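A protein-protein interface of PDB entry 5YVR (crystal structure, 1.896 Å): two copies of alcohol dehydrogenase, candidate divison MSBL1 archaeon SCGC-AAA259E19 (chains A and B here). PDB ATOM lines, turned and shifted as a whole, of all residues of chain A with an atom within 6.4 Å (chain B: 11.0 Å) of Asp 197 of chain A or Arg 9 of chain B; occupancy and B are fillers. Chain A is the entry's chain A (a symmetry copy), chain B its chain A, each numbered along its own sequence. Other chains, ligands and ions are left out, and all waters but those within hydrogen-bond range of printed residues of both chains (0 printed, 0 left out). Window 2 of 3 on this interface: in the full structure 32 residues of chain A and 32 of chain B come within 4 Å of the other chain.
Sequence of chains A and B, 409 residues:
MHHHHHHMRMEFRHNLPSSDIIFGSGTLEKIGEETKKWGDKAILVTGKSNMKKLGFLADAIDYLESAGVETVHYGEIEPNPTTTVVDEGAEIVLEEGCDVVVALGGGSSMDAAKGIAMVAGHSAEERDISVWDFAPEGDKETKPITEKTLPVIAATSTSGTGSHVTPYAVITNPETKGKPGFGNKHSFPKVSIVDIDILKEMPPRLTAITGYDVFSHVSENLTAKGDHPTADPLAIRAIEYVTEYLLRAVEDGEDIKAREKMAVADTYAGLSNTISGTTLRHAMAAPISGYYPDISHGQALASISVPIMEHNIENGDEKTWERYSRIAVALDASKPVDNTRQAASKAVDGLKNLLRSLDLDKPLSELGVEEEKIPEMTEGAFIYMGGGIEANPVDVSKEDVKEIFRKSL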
ATOM      1  N   GLY A  24      19.536  27.738  -4.688  1.00  0.00           N
ATOM      2  CA  GLY A  24      19.640  27.435  -3.275  1.00  0.00           C
ATOM      3  C   GLY A  24      18.498  28.099  -2.535  1.00  0.00           C
ATOM      4  O   GLY A  24      17.562  28.620  -3.138  1.00  0.00           O
ATOM      5  N   SER A  25      18.570  28.040  -1.219  1.00  0.00           N
ATOM      6  CA  SER A  25      17.523  28.641  -0.412  1.00  0.00           C
ATOM      7  C   SER A  25      18.104  29.914   0.186  1.00  0.00           C
ATOM      8  O   SER A  25      19.232  29.909   0.697  1.00  0.00           O
ATOM      9  CB  SER A  25      17.010  27.661   0.645  1.00  0.00           C
ATOM     10  OG  SER A  25      17.894  27.639   1.738  1.00  0.00           O
ATOM     11  N   GLY A  26      17.385  31.010   0.028  1.00  0.00           N
ATOM     12  CA  GLY A  26      17.893  32.302   0.444  1.00  0.00           C
ATOM     13  C   GLY A  26      18.756  33.016  -0.574  1.00  0.00           C
ATOM     14  O   GLY A  26      19.353  34.040  -0.228  1.00  0.00           O
ATOM     15  N   THR A  27      18.826  32.522  -1.820  1.00  0.00           N
ATOM     16  CA  THR A  27      19.593  33.187  -2.873  1.00  0.00           C
ATOM     17  C   THR A  27      18.922  34.449  -3.406  1.00  0.00           C
ATOM     18  O   THR A  27      19.541  35.165  -4.205  1.00  0.00           O
ATOM     19  CB  THR A  27      19.821  32.227  -4.025  1.00  0.00           C
ATOM     20  OG1 THR A  27      18.557  31.656  -4.408  1.00  0.00           O
ATOM     21  CG2 THR A  27      20.845  31.133  -3.603  1.00  0.00           C
ATOM     22  N   PHE A  56       8.626  38.562   0.233  1.00  0.00           N
ATOM     23  CA  PHE A  56       9.768  38.550  -0.679  1.00  0.00           C
ATOM     24  C   PHE A  56       9.839  39.833  -1.508  1.00  0.00           C
ATOM     25  O   PHE A  56      10.937  40.273  -1.861  1.00  0.00           O
ATOM     26  CB  PHE A  56       9.737  37.292  -1.568  1.00  0.00           C
ATOM     27  CG  PHE A  56       9.809  35.998  -0.778  1.00  0.00           C
ATOM     28  CD1 PHE A  56      10.945  35.698  -0.026  1.00  0.00           C
ATOM     29  CD2 PHE A  56       8.734  35.095  -0.771  1.00  0.00           C
ATOM     30  CE1 PHE A  56      11.025  34.531   0.705  1.00  0.00           C
ATOM     31  CE2 PHE A  56       8.798  33.912  -0.048  1.00  0.00           C
ATOM     32  CZ  PHE A  56       9.940  33.624   0.697  1.00  0.00           C
ATOM     33  N   ASP A 195      15.220  30.316  -5.743  1.00  0.00           N
ATOM     34  CA  ASP A 195      15.252  30.344  -4.283  1.00  0.00           C
ATOM     35  C   ASP A 195      14.198  29.391  -3.725  1.00  0.00           C
ATOM     36  O   ASP A 195      12.988  29.629  -3.881  1.00  0.00           O
ATOM     37  CB  ASP A 195      15.008  31.763  -3.759  1.00  0.00           C
ATOM     38  CG  ASP A 195      15.380  31.918  -2.317  1.00  0.00           C
ATOM     39  OD1 ASP A 195      15.297  30.915  -1.558  1.00  0.00           O
ATOM     40  OD2 ASP A 195      15.741  33.064  -1.916  1.00  0.00           O
ATOM     41  N   ILE A 196      14.657  28.359  -3.015  1.00  0.00           N
ATOM     42  CA  ILE A 196      13.737  27.336  -2.511  1.00  0.00           C
ATOM     43  C   ILE A 196      12.787  27.930  -1.469  1.00  0.00           C
ATOM     44  O   ILE A 196      11.658  27.450  -1.289  1.00  0.00           O
ATOM     45  CB  ILE A 196      14.541  26.162  -1.927  1.00  0.00           C
ATOM     46  CG1 ILE A 196      15.408  25.524  -2.998  1.00  0.00           C
ATOM     47  CG2 ILE A 196      13.618  25.167  -1.256  1.00  0.00           C
ATOM     48  CD1 ILE A 196      14.631  25.006  -4.151  1.00  0.00           C
ATOM     49  N   ASP A 197      13.220  28.981  -0.770  1.00  0.00           N
ATOM     50  CA  ASP A 197      12.353  29.597   0.228  1.00  0.00           C
ATOM     51  C   ASP A 197      11.144  30.258  -0.406  1.00  0.00           C
ATOM     52  O   ASP A 197      10.087  30.362   0.226  1.00  0.00           O
ATOM     53  CB  ASP A 197      13.155  30.584   1.051  1.00  0.00           C
ATOM     54  CG  ASP A 197      14.086  29.879   1.989  1.00  0.00           C
ATOM     55  OD1 ASP A 197      13.900  28.642   2.114  1.00  0.00           O
ATOM     56  OD2 ASP A 197      14.960  30.546   2.587  1.00  0.00           O
ATOM     57  N   ILE A 198      11.267  30.684  -1.655  1.00  0.00           N
ATOM     58  CA  ILE A 198      10.138  31.268  -2.369  1.00  0.00           C
ATOM     59  C   ILE A 198       9.254  30.178  -2.943  1.00  0.00           C
ATOM     60  O   ILE A 198       8.028  30.166  -2.743  1.00  0.00           O
ATOM     61  CB  ILE A 198      10.667  32.207  -3.470  1.00  0.00           C
ATOM     62  CG1 ILE A 198      11.527  33.328  -2.868  1.00  0.00           C
ATOM     63  CG2 ILE A 198       9.542  32.749  -4.294  1.00  0.00           C
ATOM     64  CD1 ILE A 198      12.003  34.321  -3.925  1.00  0.00           C
ATOM     65  N   LEU A 199       9.886  29.183  -3.595  1.00  0.00           N
ATOM     66  CA  LEU A 199       9.150  28.115  -4.267  1.00  0.00           C
ATOM     67  C   LEU A 199       8.326  27.282  -3.289  1.00  0.00           C
ATOM     68  O   LEU A 199       7.204  26.884  -3.611  1.00  0.00           O
ATOM     69  CB  LEU A 199      10.112  27.176  -5.022  1.00  0.00           C
ATOM     70  CG  LEU A 199      11.019  27.919  -6.005  1.00  0.00           C
ATOM     71  CD1 LEU A 199      12.131  26.920  -6.478  1.00  0.00           C
ATOM     72  CD2 LEU A 199      10.173  28.439  -7.157  1.00  0.00           C
ATOM     73  N   LYS A 200       8.873  26.991  -2.106  1.00  0.00           N
ATOM     74  CA  LYS A 200       8.194  26.115  -1.156  1.00  0.00           C
ATOM     75  C   LYS A 200       6.921  26.742  -0.611  1.00  0.00           C
ATOM     76  O   LYS A 200       6.159  26.049   0.070  1.00  0.00           O
ATOM     77  CB  LYS A 200       9.126  25.771   0.010  1.00  0.00           C
ATOM     78  CG  LYS A 200       9.125  26.877   1.085  1.00  0.00           C
ATOM     79  CD  LYS A 200      10.222  26.753   2.182  1.00  0.00           C
ATOM     80  CE  LYS A 200      10.194  27.969   3.168  1.00  0.00           C
ATOM     81  NZ  LYS A 200       9.770  27.544   4.498  1.00  0.00           N
ATOM     82  N   GLU A 201       6.668  28.021  -0.894  1.00  0.00           N
ATOM     83  CA  GLU A 201       5.394  28.627  -0.540  1.00  0.00           C
ATOM     84  C   GLU A 201       4.313  28.442  -1.593  1.00  0.00           C
ATOM     85  O   GLU A 201       3.156  28.798  -1.324  1.00  0.00           O
ATOM     86  CB  GLU A 201       5.570  30.123  -0.252  1.00  0.00           C
ATOM     87  CG  GLU A 201       6.520  30.397   0.880  1.00  0.00           C
ATOM     88  CD  GLU A 201       5.996  29.859   2.193  1.00  0.00           C
ATOM     89  OE1 GLU A 201       4.755  29.691   2.317  1.00  0.00           O
ATOM     90  OE2 GLU A 201       6.824  29.589   3.096  1.00  0.00           O
ATOM     91  N   ILE A 256      11.423  19.636   1.611  1.00  0.00           N
ATOM     92  CA  ILE A 256      12.363  20.517   0.914  1.00  0.00           C
ATOM     93  C   ILE A 256      13.089  19.754  -0.187  1.00  0.00           C
ATOM     94  O   ILE A 256      13.280  20.273  -1.301  1.00  0.00           O
ATOM     95  CB  ILE A 256      13.357  21.148   1.910  1.00  0.00           C
ATOM     96  CG1 ILE A 256      12.633  21.852   3.086  1.00  0.00           C
ATOM     97  CG2 ILE A 256      14.374  22.028   1.181  1.00  0.00           C
ATOM     98  CD1 ILE A 256      11.819  23.074   2.707  1.00  0.00           C
ATOM     99  N   GLU A 260      13.320  20.894  -3.982  1.00  0.00           N
ATOM    100  CA  GLU A 260      14.597  21.068  -4.672  1.00  0.00           C
ATOM    101  C   GLU A 260      14.620  20.283  -5.966  1.00  0.00           C
ATOM    102  O   GLU A 260      15.148  20.762  -6.973  1.00  0.00           O
ATOM    103  CB  GLU A 260      15.754  20.622  -3.782  1.00  0.00           C
ATOM    104  CG  GLU A 260      16.061  21.505  -2.609  1.00  0.00           C
ATOM    105  CD  GLU A 260      17.079  20.863  -1.678  1.00  0.00           C
ATOM    106  OE1 GLU A 260      17.334  19.666  -1.823  1.00  0.00           O
ATOM    107  OE2 GLU A 260      17.658  21.549  -0.831  1.00  0.00           O
ATOM    108  N   HIS B   7      17.469  17.273   6.655  1.00  0.00           N
ATOM    109  CA  HIS B   7      17.887  17.250   5.239  1.00  0.00           C
ATOM    110  C   HIS B   7      18.962  18.310   4.848  1.00  0.00           C
ATOM    111  O   HIS B   7      18.821  19.493   5.136  1.00  0.00           O
ATOM    112  CB  HIS B   7      16.650  17.417   4.347  1.00  0.00           C
ATOM    113  CG  HIS B   7      16.960  17.664   2.902  1.00  0.00           C
ATOM    114  ND1 HIS B   7      17.437  16.680   2.060  1.00  0.00           N
ATOM    115  CD2 HIS B   7      16.870  18.786   2.147  1.00  0.00           C
ATOM    116  CE1 HIS B   7      17.629  17.183   0.851  1.00  0.00           C
ATOM    117  NE2 HIS B   7      17.295  18.462   0.876  1.00  0.00           N
ATOM    118  N   MET B   8      20.023  17.869   4.163  1.00  0.00           N
ATOM    119  CA  MET B   8      21.072  18.760   3.662  1.00  0.00           C
ATOM    120  C   MET B   8      20.589  19.571   2.451  1.00  0.00           C
ATOM    121  O   MET B   8      20.293  19.007   1.392  1.00  0.00           O
ATOM    122  CB  MET B   8      22.299  17.940   3.277  1.00  0.00           C
ATOM    123  CG  MET B   8      22.962  17.181   4.423  1.00  0.00           C
ATOM    124  SD  MET B   8      24.544  16.431   3.936  1.00  0.00           S
ATOM    125  CE  MET B   8      25.127  17.585   2.679  1.00  0.00           C
ATOM    126  N   ARG B   9      20.528  20.894   2.591  1.00  0.00           N
ATOM    127  CA  ARG B   9      20.035  21.698   1.490  1.00  0.00           C
ATOM    128  C   ARG B   9      21.005  21.645   0.307  1.00  0.00           C
ATOM    129  O   ARG B   9      22.176  21.290   0.436  1.00  0.00           O
ATOM    130  CB  ARG B   9      19.814  23.141   1.924  1.00  0.00           C
ATOM    131  CG  ARG B   9      18.764  23.288   2.994  1.00  0.00           C
ATOM    132  CD  ARG B   9      17.468  23.933   2.493  1.00  0.00           C
ATOM    133  NE  ARG B   9      16.511  24.099   3.594  1.00  0.00           N
ATOM    134  CZ  ARG B   9      15.393  24.827   3.546  1.00  0.00           C
ATOM    135  NH1 ARG B   9      15.060  25.498   2.438  1.00  0.00           N
ATOM    136  NH2 ARG B   9      14.609  24.908   4.624  1.00  0.00           N
ATOM    137  N   MET B  10      20.479  21.963  -0.861  1.00  0.00           N
ATOM    138  CA  MET B  10      21.230  21.939  -2.102  1.00  0.00           C
ATOM    139  C   MET B  10      21.566  23.377  -2.485  1.00  0.00           C
ATOM    140  O   MET B  10      20.701  24.266  -2.426  1.00  0.00           O
ATOM    141  CB  MET B  10      20.434  21.243  -3.207  1.00  0.00           C
ATOM    142  CG  MET B  10      21.218  20.999  -4.479  1.00  0.00           C
ATOM    143  SD  MET B  10      20.145  20.489  -5.850  1.00  0.00           S
ATOM    144  CE  MET B  10      19.268  19.066  -5.173  1.00  0.00           C
ATOM    145  N   GLU B  11      22.831  23.608  -2.830  1.00  0.00           N
ATOM    146  CA  GLU B  11      23.319  24.923  -3.214  1.00  0.00           C
ATOM    147  C   GLU B  11      24.284  24.758  -4.376  1.00  0.00           C
ATOM    148  O   GLU B  11      25.178  23.910  -4.311  1.00  0.00           O
ATOM    149  CB  GLU B  11      24.032  25.603  -2.044  1.00  0.00           C
ATOM    150  CG  GLU B  11      23.137  26.398  -1.129  1.00  0.00           C
ATOM    151  CD  GLU B  11      23.473  27.894  -1.155  1.00  0.00           C
ATOM    152  OE1 GLU B  11      22.584  28.711  -0.781  1.00  0.00           O
ATOM    153  OE2 GLU B  11      24.625  28.244  -1.560  1.00  0.00           O
ATOM    154  N   PHE B  12      24.115  25.547  -5.433  1.00  0.00           N
ATOM    155  CA  PHE B  12      25.148  25.593  -6.469  1.00  0.00           C
ATOM    156  C   PHE B  12      24.946  26.821  -7.332  1.00  0.00           C
ATOM    157  O   PHE B  12      23.888  27.456  -7.309  1.00  0.00           O
ATOM    158  CB  PHE B  12      25.141  24.354  -7.372  1.00  0.00           C
ATOM    159  CG  PHE B  12      23.855  24.159  -8.121  1.00  0.00           C
ATOM    160  CD1 PHE B  12      22.753  23.560  -7.493  1.00  0.00           C
ATOM    161  CD2 PHE B  12      23.726  24.599  -9.428  1.00  0.00           C
ATOM    162  CE1 PHE B  12      21.545  23.391  -8.148  1.00  0.00           C
ATOM    163  CE2 PHE B  12      22.520  24.437 -10.108  1.00  0.00           C
ATOM    164  CZ  PHE B  12      21.422  23.800  -9.464  1.00  0.00           C
ATOM    165  N   GLY B 226      30.606  18.949  -4.021  1.00  0.00           N
ATOM    166  CA  GLY B 226      29.437  19.819  -4.111  1.00  0.00           C
ATOM    167  C   GLY B 226      28.414  19.295  -5.095  1.00  0.00           C
ATOM    168  O   GLY B 226      28.607  18.277  -5.781  1.00  0.00           O
ATOM    169  N   ASP B 227      27.300  20.021  -5.167  1.00  0.00           N
ATOM    170  CA  ASP B 227      26.210  19.733  -6.086  1.00  0.00           C
ATOM    171  C   ASP B 227      26.454  20.374  -7.441  1.00  0.00           C
ATOM    172  O   ASP B 227      26.848  21.537  -7.510  1.00  0.00           O
ATOM    173  CB  ASP B 227      24.910  20.276  -5.519  1.00  0.00           C
ATOM    174  CG  ASP B 227      24.507  19.555  -4.231  1.00  0.00           C
ATOM    175  OD1 ASP B 227      24.592  18.308  -4.245  1.00  0.00           O
ATOM    176  OD2 ASP B 227      24.205  20.234  -3.237  1.00  0.00           O
ATOM    177  N   HIS B 228      26.129  19.640  -8.515  1.00  0.00           N
ATOM    178  CA  HIS B 228      26.226  20.163  -9.887  1.00  0.00           C
ATOM    179  C   HIS B 228      25.187  19.433 -10.738  1.00  0.00           C
ATOM    180  O   HIS B 228      25.529  18.715 -11.685  1.00  0.00           O
ATOM    181  CB  HIS B 228      27.646  19.988 -10.453  1.00  0.00           C
ATOM    182  CG  HIS B 228      28.387  18.820  -9.857  1.00  0.00           C
ATOM    183  ND1 HIS B 228      28.105  17.508 -10.185  1.00  0.00           N
ATOM    184  CD2 HIS B 228      29.357  18.767  -8.914  1.00  0.00           C
ATOM    185  CE1 HIS B 228      28.893  16.694  -9.500  1.00  0.00           C
ATOM    186  NE2 HIS B 228      29.661  17.431  -8.713  1.00  0.00           N
ATOM    187  N   PRO B 229      23.899  19.595 -10.442  1.00  0.00           N
ATOM    188  CA  PRO B 229      22.905  18.718 -11.083  1.00  0.00           C
ATOM    189  C   PRO B 229      22.698  19.014 -12.557  1.00  0.00           C
ATOM    190  O   PRO B 229      22.195  18.143 -13.277  1.00  0.00           O
ATOM    191  CB  PRO B 229      21.630  18.956 -10.257  1.00  0.00           C
ATOM    192  CG  PRO B 229      21.816  20.292  -9.672  1.00  0.00           C
ATOM    193  CD  PRO B 229      23.294  20.496  -9.451  1.00  0.00           C
ATOM    194  N   LYS B 319      27.486  10.031   0.120  1.00  0.00           N
ATOM    195  CA  LYS B 319      27.124  10.804  -1.069  1.00  0.00           C
ATOM    196  C   LYS B 319      28.106  10.557  -2.227  1.00  0.00           C
ATOM    197  O   LYS B 319      27.692  10.429  -3.385  1.00  0.00           O
ATOM    198  CB  LYS B 319      27.058  12.286  -0.720  1.00  0.00           C
ATOM    199  CG  LYS B 319      26.714  13.173  -1.917  1.00  0.00           C
ATOM    200  CD  LYS B 319      26.788  14.633  -1.531  1.00  0.00           C
ATOM    201  CE  LYS B 319      26.422  15.523  -2.684  1.00  0.00           C
ATOM    202  NZ  LYS B 319      26.730  16.952  -2.423  1.00  0.00           N
ATOM    203  N   ARG B 323      27.570   8.351  -5.954  1.00  0.00           N
ATOM    204  CA  ARG B 323      28.024   8.778  -7.276  1.00  0.00           C
ATOM    205  C   ARG B 323      28.850   7.686  -7.972  1.00  0.00           C
ATOM    206  O   ARG B 323      28.580   7.328  -9.126  1.00  0.00           O
ATOM    207  CB  ARG B 323      28.803  10.099  -7.162  1.00  0.00           C
ATOM    208  CG  ARG B 323      27.882  11.312  -6.984  1.00  0.00           C
ATOM    209  CD  ARG B 323      28.542  12.455  -6.223  1.00  0.00           C
ATOM    210  NE  ARG B 323      27.743  13.682  -6.392  1.00  0.00           N
ATOM    211  CZ  ARG B 323      28.171  14.911  -6.112  1.00  0.00           C
ATOM    212  NH1 ARG B 323      29.400  15.082  -5.638  1.00  0.00           N
ATOM    213  NH2 ARG B 323      27.385  15.974  -6.338  1.00  0.00           N
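Of the 14 printed residues of chain A, 6 touch a printed residue of chain B. Hydrophobic or aromatic side chains of chain A that line the printed part of chain B: Ile 196 and Ile 256. Of the 12 printed residues of chain B, 4 touch a printed residue of chain A. Printed residues of chain B that touch a printed residue of chain A: His 7, Arg 9, Met 10 and Glu 11. Hydrophobic or aromatic side chains of chain B that line the printed part of chain A: His 7 and Met 10. Among the printed residues, 9 pairs touch across the chains.
No position is printed for both chains. Of the 9 pairs that touch across the chains among the printed residues, none has its exchanged pair printed and touching as well.
Gly 24 of chain A touches Met 10 of chain B. CB of Ser 25 of chain A touches NH1 of Arg 9 of chain B, at 3.4 Å. OE1 of Glu 11 of chain B touches O of Ser 25 of chain A, 3.9 Å away. CG2 of Ile 196 of chain A touches NH1 of Arg 9 of chain B (3.98 Å). CG2 of Ile 256 of chain A touches NH1 of Arg 9 of chain B (3.8 Å). Arg 9 of chain B touches Glu 260 of chain A.
Asp 197 of chain A touches one residue of chain B. Asp 195 of chain A touches none of the printed residues of chain B. Ile 196 of chain A touches just one residue of chain B: Arg 9 (3.98 Å). No residue of chain B comes within 4 Å of Ile 198 of chain A. No residue of chain B comes within 4 Å of Lys 200 of chain A. Ile 256 of chain A touches one residue of chain B. Printed residues of chain B within 4 Å of Gly 24 of chain A: Met 10 (3.4 Å). Of the printed residues of chain A, Met 10 of chain B touches Gly 24 (3.4 Å) and Glu 260 (2.9 Å). Printed residues of chain B within 4 Å of Glu 260 of chain A: His 7 (3.0 Å), Arg 9 (3.3 Å) and Met 10 (2.9 Å). Phe 12 of chain B touches none of the printed residues of chain A. Gly 226 of chain B touches none of the printed residues of chain A. The nearest residue of chain A that does not touch Arg 9 of chain B is Lys 200 of chain A (5.0 Å). The nearest printed residue of chain A that does not touch His 7 of chain B is Ile 256 of chain A (4.2 Å).
The backbone carbonyl oxygen (O) of Gly 24 of chain A sits at hydrogen-bond distance from the side-chain hydroxyl (OG1) of Thr 27 of chain A (3.4 Å). O of Gly 24 of chain A lies within hydrogen-bond range of N of Ile 196 of chain A (2.9 Å). The backbone NH (N) of Asp 197 of chain A lies within hydrogen-bond range of the side-chain carboxylate (OD1) of Asp 195 of chain A, 2.9 Å away.
A ring nitrogen (NE2) of His 7 of chain B sits at hydrogen-bond distance from the side-chain carboxylate (OE1) of Glu 260 of chain A (3.0 Å). NH1 of Arg 9 of chain B is in salt-bridge range of OD1 of Asp 197 of chain A. The backbone NH (N) of Met 10 of chain B sits at hydrogen-bond distance from the side-chain carboxylate (OE2) of Glu 260 of chain A, at 2.9 Å.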
